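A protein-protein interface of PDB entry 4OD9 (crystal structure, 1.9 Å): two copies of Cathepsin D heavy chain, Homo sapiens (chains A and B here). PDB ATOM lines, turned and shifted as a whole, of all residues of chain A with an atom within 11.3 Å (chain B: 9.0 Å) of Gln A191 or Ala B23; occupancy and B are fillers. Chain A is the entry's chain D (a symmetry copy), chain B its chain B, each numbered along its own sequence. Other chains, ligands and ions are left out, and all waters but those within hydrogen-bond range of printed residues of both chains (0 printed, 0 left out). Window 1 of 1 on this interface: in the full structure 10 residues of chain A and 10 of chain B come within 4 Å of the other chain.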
ATOM      1  N   LEU A 151      -6.617 -16.551  18.987  1.00  0.00           N
ATOM      2  CA  LEU A 151      -6.292 -17.408  17.850  1.00  0.00           C
ATOM      3  C   LEU A 151      -4.811 -17.170  17.508  1.00  0.00           C
ATOM      4  O   LEU A 151      -3.975 -17.991  17.853  1.00  0.00           O
ATOM      5  CB  LEU A 151      -7.213 -17.110  16.650  1.00  0.00           C
ATOM      6  CG  LEU A 151      -6.936 -17.875  15.335  1.00  0.00           C
ATOM      7  CD1 LEU A 151      -7.296 -19.357  15.459  1.00  0.00           C
ATOM      8  CD2 LEU A 151      -7.707 -17.251  14.161  1.00  0.00           C
ATOM      9  N   ILE A 152      -4.502 -16.053  16.833  1.00  0.00           N
ATOM     10  CA  ILE A 152      -3.157 -15.637  16.406  1.00  0.00           C
ATOM     11  C   ILE A 152      -3.230 -14.168  16.022  1.00  0.00           C
ATOM     12  O   ILE A 152      -4.284 -13.713  15.555  1.00  0.00           O
ATOM     13  CB  ILE A 152      -2.558 -16.442  15.193  1.00  0.00           C
ATOM     14  CG1 ILE A 152      -3.524 -16.485  13.970  1.00  0.00           C
ATOM     15  CG2 ILE A 152      -2.025 -17.811  15.563  1.00  0.00           C
ATOM     16  CD1 ILE A 152      -2.809 -16.741  12.575  1.00  0.00           C
ATOM     17  N   GLU A 155      -6.204 -11.751  16.699  1.00  0.00           N
ATOM     18  CA  GLU A 155      -7.510 -12.330  16.366  1.00  0.00           C
ATOM     19  C   GLU A 155      -7.928 -13.341  17.423  1.00  0.00           C
ATOM     20  O   GLU A 155      -7.083 -13.937  18.104  1.00  0.00           O
ATOM     21  CB  GLU A 155      -7.500 -12.989  14.980  1.00  0.00           C
ATOM     22  CG  GLU A 155      -7.468 -11.973  13.845  1.00  0.00           C
ATOM     23  CD  GLU A 155      -7.468 -12.513  12.427  1.00  0.00           C
ATOM     24  OE1 GLU A 155      -7.829 -13.694  12.219  1.00  0.00           O
ATOM     25  OE2 GLU A 155      -7.098 -11.742  11.513  1.00  0.00           O
ATOM     26  N   TYR A 156      -9.258 -13.489  17.583  1.00  0.00           N
ATOM     27  CA  TYR A 156      -9.889 -14.351  18.588  1.00  0.00           C
ATOM     28  C   TYR A 156     -11.016 -15.166  17.954  1.00  0.00           C
ATOM     29  O   TYR A 156     -11.624 -14.710  16.982  1.00  0.00           O
ATOM     30  CB  TYR A 156     -10.501 -13.482  19.702  1.00  0.00           C
ATOM     31  CG  TYR A 156      -9.501 -12.729  20.554  1.00  0.00           C
ATOM     32  CD1 TYR A 156      -8.913 -11.545  20.095  1.00  0.00           C
ATOM     33  CD2 TYR A 156      -9.229 -13.130  21.863  1.00  0.00           C
ATOM     34  CE1 TYR A 156      -8.029 -10.817  20.892  1.00  0.00           C
ATOM     35  CE2 TYR A 156      -8.353 -12.398  22.677  1.00  0.00           C
ATOM     36  CZ  TYR A 156      -7.742 -11.254  22.174  1.00  0.00           C
ATOM     37  OH  TYR A 156      -6.909 -10.496  22.948  1.00  0.00           O
ATOM     38  N   MET A 157     -11.299 -16.354  18.518  1.00  0.00           N
ATOM     39  CA  MET A 157     -12.389 -17.235  18.071  1.00  0.00           C
ATOM     40  C   MET A 157     -13.406 -17.359  19.200  1.00  0.00           C
ATOM     41  O   MET A 157     -13.033 -17.321  20.370  1.00  0.00           O
ATOM     42  CB  MET A 157     -11.857 -18.640  17.709  1.00  0.00           C
ATOM     43  CG  MET A 157     -11.036 -18.702  16.453  1.00  0.00           C
ATOM     44  SD  MET A 157     -12.038 -18.668  14.952  1.00  0.00           S
ATOM     45  CE  MET A 157     -10.850 -19.255  13.773  1.00  0.00           C
ATOM     46  N   ILE A 158     -14.673 -17.572  18.862  1.00  0.00           N
ATOM     47  CA  ILE A 158     -15.733 -17.750  19.863  1.00  0.00           C
ATOM     48  C   ILE A 158     -16.401 -19.097  19.566  1.00  0.00           C
ATOM     49  O   ILE A 158     -16.752 -19.307  18.406  1.00  0.00           O
ATOM     50  CB  ILE A 158     -16.810 -16.597  19.784  1.00  0.00           C
ATOM     51  CG1 ILE A 158     -16.177 -15.207  19.933  1.00  0.00           C
ATOM     52  CG2 ILE A 158     -17.957 -16.798  20.828  1.00  0.00           C
ATOM     53  CD1 ILE A 158     -16.823 -14.125  19.071  1.00  0.00           C
ATOM     54  N   CYS A 160     -18.967 -21.445  18.413  1.00  0.00           N
ATOM     55  CA  CYS A 160     -20.147 -21.137  17.601  1.00  0.00           C
ATOM     56  C   CYS A 160     -21.487 -21.259  18.347  1.00  0.00           C
ATOM     57  O   CYS A 160     -22.396 -20.473  18.079  1.00  0.00           O
ATOM     58  CB  CYS A 160     -20.146 -21.963  16.321  1.00  0.00           C
ATOM     59  SG  CYS A 160     -18.903 -21.434  15.118  1.00  0.00           S
ATOM     60  N   LEU A 187     -17.819 -13.740  12.358  1.00  0.00           N
ATOM     61  CA  LEU A 187     -17.645 -14.223  10.989  1.00  0.00           C
ATOM     62  C   LEU A 187     -17.581 -15.732  11.011  1.00  0.00           C
ATOM     63  O   LEU A 187     -16.814 -16.293  11.782  1.00  0.00           O
ATOM     64  CB  LEU A 187     -16.324 -13.680  10.403  1.00  0.00           C
ATOM     65  CG  LEU A 187     -16.296 -12.220   9.977  1.00  0.00           C
ATOM     66  CD1 LEU A 187     -15.830 -11.302  11.125  1.00  0.00           C
ATOM     67  CD2 LEU A 187     -15.386 -12.054   8.769  1.00  0.00           C
ATOM     68  N   LYS A 188     -18.369 -16.396  10.176  1.00  0.00           N
ATOM     69  CA  LYS A 188     -18.333 -17.853  10.097  1.00  0.00           C
ATOM     70  C   LYS A 188     -17.234 -18.227   9.110  1.00  0.00           C
ATOM     71  O   LYS A 188     -17.302 -17.832   7.950  1.00  0.00           O
ATOM     72  CB  LYS A 188     -19.698 -18.434   9.683  1.00  0.00           C
ATOM     73  CG  LYS A 188     -20.709 -18.436  10.823  1.00  0.00           C
ATOM     74  CD  LYS A 188     -21.615 -19.660  10.792  1.00  0.00           C
ATOM     75  CE  LYS A 188     -22.388 -19.789  12.090  1.00  0.00           C
ATOM     76  NZ  LYS A 188     -22.493 -21.202  12.572  1.00  0.00           N
ATOM     77  N   VAL A 189     -16.180 -18.901   9.597  1.00  0.00           N
ATOM     78  CA  VAL A 189     -15.038 -19.324   8.785  1.00  0.00           C
ATOM     79  C   VAL A 189     -15.019 -20.847   8.645  1.00  0.00           C
ATOM     80  O   VAL A 189     -15.314 -21.566   9.609  1.00  0.00           O
ATOM     81  CB  VAL A 189     -13.685 -18.729   9.281  1.00  0.00           C
ATOM     82  CG1 VAL A 189     -13.239 -19.343  10.605  1.00  0.00           C
ATOM     83  CG2 VAL A 189     -12.587 -18.853   8.225  1.00  0.00           C
ATOM     84  N   SER A 190     -14.735 -21.335   7.432  1.00  0.00           N
ATOM     85  CA  SER A 190     -14.648 -22.770   7.194  1.00  0.00           C
ATOM     86  C   SER A 190     -13.348 -23.128   6.506  1.00  0.00           C
ATOM     87  O   SER A 190     -13.071 -22.642   5.403  1.00  0.00           O
ATOM     88  CB  SER A 190     -15.872 -23.307   6.452  1.00  0.00           C
ATOM     89  OG  SER A 190     -15.862 -22.983   5.071  1.00  0.00           O
ATOM     90  N   GLN A 191     -12.518 -23.923   7.196  1.00  0.00           N
ATOM     91  CA  GLN A 191     -11.243 -24.397   6.666  1.00  0.00           C
ATOM     92  C   GLN A 191     -11.205 -25.928   6.742  1.00  0.00           C
ATOM     93  O   GLN A 191     -11.506 -26.497   7.799  1.00  0.00           O
ATOM     94  CB  GLN A 191     -10.034 -23.685   7.325  1.00  0.00           C
ATOM     95  CG  GLN A 191      -9.546 -24.226   8.673  1.00  0.00           C
ATOM     96  CD  GLN A 191     -10.425 -23.927   9.857  1.00  0.00           C
ATOM     97  OE1 GLN A 191     -11.454 -24.574  10.086  1.00  0.00           O
ATOM     98  NE2 GLN A 191      -9.972 -23.008  10.697  1.00  0.00           N
ATOM     99  N   ALA A 192     -10.904 -26.588   5.598  1.00  0.00           N
ATOM    100  CA  ALA A 192     -10.899 -28.055   5.438  1.00  0.00           C
ATOM    101  C   ALA A 192     -12.226 -28.690   5.928  1.00  0.00           C
ATOM    102  O   ALA A 192     -12.222 -29.658   6.694  1.00  0.00           O
ATOM    103  CB  ALA A 192      -9.691 -28.676   6.127  1.00  0.00           C
ATOM    104  N   GLY A 193     -13.340 -28.084   5.501  1.00  0.00           N
ATOM    105  CA  GLY A 193     -14.701 -28.498   5.833  1.00  0.00           C
ATOM    106  C   GLY A 193     -15.042 -28.464   7.310  1.00  0.00           C
ATOM    107  O   GLY A 193     -15.751 -29.351   7.801  1.00  0.00           O
ATOM    108  N   LYS A 194     -14.523 -27.448   8.036  1.00  0.00           N
ATOM    109  CA  LYS A 194     -14.751 -27.280   9.483  1.00  0.00           C
ATOM    110  C   LYS A 194     -15.234 -25.870   9.768  1.00  0.00           C
ATOM    111  O   LYS A 194     -14.581 -24.917   9.337  1.00  0.00           O
ATOM    112  CB  LYS A 194     -13.471 -27.572  10.281  1.00  0.00           C
ATOM    113  CG  LYS A 194     -13.004 -29.006  10.162  1.00  0.00           C
ATOM    114  CD  LYS A 194     -11.496 -29.092  10.063  1.00  0.00           C
ATOM    115  CE  LYS A 194     -10.941 -29.906  11.198  1.00  0.00           C
ATOM    116  NZ  LYS A 194     -11.440 -31.312  11.194  1.00  0.00           N
ATOM    117  N   THR A 195     -16.353 -25.731  10.512  1.00  0.00           N
ATOM    118  CA  THR A 195     -16.957 -24.417  10.814  1.00  0.00           C
ATOM    119  C   THR A 195     -16.539 -23.818  12.183  1.00  0.00           C
ATOM    120  O   THR A 195     -16.897 -24.346  13.244  1.00  0.00           O
ATOM    121  CB  THR A 195     -18.498 -24.480  10.667  1.00  0.00           C
ATOM    122  OG1 THR A 195     -18.834 -25.012   9.380  1.00  0.00           O
ATOM    123  CG2 THR A 195     -19.166 -23.116  10.840  1.00  0.00           C
ATOM    124  N   LEU A 196     -15.846 -22.653  12.128  1.00  0.00           N
ATOM    125  CA  LEU A 196     -15.450 -21.892  13.319  1.00  0.00           C
ATOM    126  C   LEU A 196     -15.997 -20.486  13.238  1.00  0.00           C
ATOM    127  O   LEU A 196     -16.280 -19.993  12.144  1.00  0.00           O
ATOM    128  CB  LEU A 196     -13.924 -21.827  13.492  1.00  0.00           C
ATOM    129  CG  LEU A 196     -13.230 -23.118  13.895  1.00  0.00           C
ATOM    130  CD1 LEU A 196     -11.760 -22.982  13.695  1.00  0.00           C
ATOM    131  CD2 LEU A 196     -13.562 -23.505  15.325  1.00  0.00           C
ATOM    132  N   CYS A 197     -16.147 -19.837  14.391  1.00  0.00           N
ATOM    133  CA  CYS A 197     -16.683 -18.488  14.438  1.00  0.00           C
ATOM    134  C   CYS A 197     -15.604 -17.523  14.911  1.00  0.00           C
ATOM    135  O   CYS A 197     -15.142 -17.602  16.051  1.00  0.00           O
ATOM    136  CB  CYS A 197     -17.932 -18.446  15.309  1.00  0.00           C
ATOM    137  SG  CYS A 197     -19.294 -19.474  14.678  1.00  0.00           S
ATOM    138  N   LEU A 198     -15.176 -16.654  14.007  1.00  0.00           N
ATOM    139  CA  LEU A 198     -14.147 -15.654  14.281  1.00  0.00           C
ATOM    140  C   LEU A 198     -14.761 -14.393  14.909  1.00  0.00           C
ATOM    141  O   LEU A 198     -15.795 -13.901  14.434  1.00  0.00           O
ATOM    142  CB  LEU A 198     -13.428 -15.292  12.954  1.00  0.00           C
ATOM    143  CG  LEU A 198     -12.321 -14.239  13.016  1.00  0.00           C
ATOM    144  CD1 LEU A 198     -11.038 -14.814  13.639  1.00  0.00           C
ATOM    145  CD2 LEU A 198     -12.013 -13.682  11.616  1.00  0.00           C
ATOM    146  N   GLY B  18      -1.041 -22.614  19.047  1.00  0.00           N
ATOM    147  CA  GLY B  18      -0.857 -22.248  17.652  1.00  0.00           C
ATOM    148  C   GLY B  18      -2.027 -22.709  16.814  1.00  0.00           C
ATOM    149  O   GLY B  18      -3.073 -23.079  17.347  1.00  0.00           O
ATOM    150  N   ILE B  19      -1.861 -22.680  15.502  1.00  0.00           N
ATOM    151  CA  ILE B  19      -2.942 -23.013  14.575  1.00  0.00           C
ATOM    152  C   ILE B  19      -2.782 -24.377  13.923  1.00  0.00           C
ATOM    153  O   ILE B  19      -3.686 -24.799  13.227  1.00  0.00           O
ATOM    154  CB  ILE B  19      -3.126 -21.900  13.508  1.00  0.00           C
ATOM    155  CG1 ILE B  19      -1.849 -21.716  12.641  1.00  0.00           C
ATOM    156  CG2 ILE B  19      -3.605 -20.599  14.150  1.00  0.00           C
ATOM    157  CD1 ILE B  19      -2.091 -21.248  11.236  1.00  0.00           C
ATOM    158  N   THR B  20      -1.636 -25.038  14.137  1.00  0.00           N
ATOM    159  CA  THR B  20      -1.191 -26.320  13.575  1.00  0.00           C
ATOM    160  C   THR B  20      -2.306 -27.331  13.383  1.00  0.00           C
ATOM    161  O   THR B  20      -2.584 -27.779  12.266  1.00  0.00           O
ATOM    162  CB  THR B  20      -0.141 -26.926  14.519  1.00  0.00           C
ATOM    163  OG1 THR B  20       0.701 -25.893  15.038  1.00  0.00           O
ATOM    164  CG2 THR B  20       0.647 -28.071  13.885  1.00  0.00           C
ATOM    165  N   PHE B  21      -2.964 -27.654  14.487  1.00  0.00           N
ATOM    166  CA  PHE B  21      -3.971 -28.693  14.530  1.00  0.00           C
ATOM    167  C   PHE B  21      -5.392 -28.217  14.272  1.00  0.00           C
ATOM    168  O   PHE B  21      -6.286 -29.052  14.127  1.00  0.00           O
ATOM    169  CB  PHE B  21      -3.856 -29.458  15.860  1.00  0.00           C
ATOM    170  CG  PHE B  21      -2.526 -30.178  15.966  1.00  0.00           C
ATOM    171  CD1 PHE B  21      -2.264 -31.308  15.196  1.00  0.00           C
ATOM    172  CD2 PHE B  21      -1.528 -29.708  16.815  1.00  0.00           C
ATOM    173  CE1 PHE B  21      -1.017 -31.949  15.266  1.00  0.00           C
ATOM    174  CE2 PHE B  21      -0.284 -30.358  16.889  1.00  0.00           C
ATOM    175  CZ  PHE B  21      -0.039 -31.473  16.111  1.00  0.00           C
ATOM    176  N   ILE B  22      -5.608 -26.915  14.135  1.00  0.00           N
ATOM    177  CA  ILE B  22      -6.962 -26.409  13.905  1.00  0.00           C
ATOM    178  C   ILE B  22      -7.517 -26.866  12.551  1.00  0.00           C
ATOM    179  O   ILE B  22      -8.547 -27.529  12.534  1.00  0.00           O
ATOM    180  CB  ILE B  22      -7.086 -24.859  14.111  1.00  0.00           C
ATOM    181  CG1 ILE B  22      -6.608 -24.443  15.509  1.00  0.00           C
ATOM    182  CG2 ILE B  22      -8.543 -24.416  13.884  1.00  0.00           C
ATOM    183  CD1 ILE B  22      -6.527 -22.934  15.729  1.00  0.00           C
ATOM    184  N   ALA B  23      -6.822 -26.545  11.443  1.00  0.00           N
ATOM    185  CA  ALA B  23      -7.279 -26.905  10.103  1.00  0.00           C
ATOM    186  C   ALA B  23      -7.089 -28.379   9.739  1.00  0.00           C
ATOM    187  O   ALA B  23      -7.882 -28.871   8.936  1.00  0.00           O
ATOM    188  CB  ALA B  23      -6.637 -26.007   9.049  1.00  0.00           C
ATOM    189  N   ALA B  24      -6.097 -29.098  10.362  1.00  0.00           N
ATOM    190  CA  ALA B  24      -5.814 -30.533  10.099  1.00  0.00           C
ATOM    191  C   ALA B  24      -7.061 -31.369  10.073  1.00  0.00           C
ATOM    192  O   ALA B  24      -7.924 -31.182  10.938  1.00  0.00           O
ATOM    193  CB  ALA B  24      -4.829 -31.084  11.128  1.00  0.00           C
ATOM    194  N   LYS B  25      -7.211 -32.247   9.051  1.00  0.00           N
ATOM    195  CA  LYS B  25      -8.407 -33.080   8.906  1.00  0.00           C
ATOM    196  C   LYS B  25      -8.497 -34.152   9.979  1.00  0.00           C
ATOM    197  O   LYS B  25      -9.594 -34.537  10.363  1.00  0.00           O
ATOM    198  CB  LYS B  25      -8.487 -33.745   7.505  1.00  0.00           C
ATOM    199  CG  LYS B  25      -9.014 -32.867   6.376  1.00  0.00           C
ATOM    200  CD  LYS B  25     -10.518 -33.001   6.210  1.00  0.00           C
ATOM    201  CE  LYS B  25     -10.988 -32.224   5.000  1.00  0.00           C
ATOM    202  NZ  LYS B  25     -12.473 -32.164   4.927  1.00  0.00           N
ATOM    203  N   PHE B  26      -7.347 -34.622  10.457  1.00  0.00           N
ATOM    204  CA  PHE B  26      -7.231 -35.698  11.441  1.00  0.00           C
ATOM    205  C   PHE B  26      -7.352 -35.233  12.894  1.00  0.00           C
ATOM    206  O   PHE B  26      -7.082 -34.070  13.195  1.00  0.00           O
ATOM    207  CB  PHE B  26      -5.912 -36.471  11.213  1.00  0.00           C
ATOM    208  CG  PHE B  26      -4.674 -35.602  11.353  1.00  0.00           C
ATOM    209  CD1 PHE B  26      -4.119 -35.346  12.600  1.00  0.00           C
ATOM    210  CD2 PHE B  26      -4.126 -34.951  10.240  1.00  0.00           C
ATOM    211  CE1 PHE B  26      -3.010 -34.486  12.727  1.00  0.00           C
ATOM    212  CE2 PHE B  26      -2.977 -34.167  10.364  1.00  0.00           C
ATOM    213  CZ  PHE B  26      -2.432 -33.931  11.603  1.00  0.00           C
ATOM    214  N   ASP B  27      -7.690 -36.176  13.802  1.00  0.00           N
ATOM    215  CA  ASP B  27      -7.781 -35.925  15.253  1.00  0.00           C
ATOM    216  C   ASP B  27      -6.439 -36.049  15.976  1.00  0.00           C
ATOM    217  O   ASP B  27      -6.126 -35.250  16.854  1.00  0.00           O
ATOM    218  CB  ASP B  27      -8.780 -36.895  15.903  1.00  0.00           C
ATOM    219  CG  ASP B  27     -10.181 -36.772  15.354  1.00  0.00           C
ATOM    220  OD1 ASP B  27     -10.673 -35.618  15.228  1.00  0.00           O
ATOM    221  OD2 ASP B  27     -10.791 -37.826  15.037  1.00  0.00           O
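O of Leu A196 is in hydrogen-bond range of N of Val A189, at 2.8 Å.
The side-chain amide oxygen (OE1) of Gln A191 sits close to the backbone carbonyl oxygen (O) of Lys A194, 3.2 Å away.
The side-chain sulfur of Cys A160 is disulfide-bonded to the side-chain sulfur of Cys A197, 2.0 Å away.
Of the 19 printed residues of chain A, 6 touch a printed residue of chain B.
Hydrophobic or aromatic side chains of chain A that line the printed part of chain B: Leu A151, Ile A152, Ala A192 and Leu A196.
Of the 10 printed residues of chain B, 5 touch a printed residue of chain A.
Hydrophobic or aromatic side chains of chain B that line the printed part of chain A: Ile B19, Ile B22 and Ala B23.
Along chain B the printed residues that touch a printed residue of chain A span positions 19 to 25.
Among the printed residues, 11 pairs touch across the chains.
Among the printed residues, no Asp or Glu carboxylate lies within 4 Å of a Lys or Arg side-chain nitrogen of the other chain.
Among the printed residues, pairs that only touch across the chains: Leu A151 with Ile B22 (3.7 Å), Ile A152 with Ile B19 (3.5 Å), Gln A191 with Ile B22 (3.8 Å), Gln A191 with Ala B23 (3.4 Å), Ala A192 with Ala B23 (3.3 Å), Lys A194 with Ile B22 (3.6 Å), Lys A194 with Ala B23 (3.8 Å), Lys A194 with Ala B24 (3.3 Å), Lys A194 with Lys B25 (3.8 Å) and Leu A196 with Ile B22 (3.5 Å).
The side-chain amino group (NZ) of Lys B25 lies within hydrogen-bond range of the backbone carbonyl oxygen (O) of Ala A192.
No position is printed for both chains.
Of the 11 pairs that touch across the chains among the printed residues, none has its exchanged pair printed and touching as well.
Printed residues of chain B within 4 Å of Leu A151: Ile B22.
Of the printed residues of chain B, Ile A152 touches Ile B19 (3.5 Å).
Leu A187 touches none of the printed residues of chain B.
Lys A188 touches none of the printed residues of chain B.
No residue of chain B comes within 4 Å of Ser A190.
Of chain B, only Ile B22 and Ala B23 come within 4 Å of Gln A191.
Of the printed residues of chain B, Leu A196 touches Ile B22.
Of the printed residues of chain A, Ile B19 touches Ile A152.
Ile B22 touches four residues of chain A.
Of chain A, only Gln A191, Ala A192 and Lys A194 come within 4 Å of Ala B23.
Of chain A, only Ala A192 and Lys A194 come within 4 Å of Lys B25.
The nearest residue of chain B that does not touch Gln A191 is Ala B24 (6.2 Å).
The nearest printed residue of chain B that does not touch Ile A152 is Gly B18 (5.0 Å).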
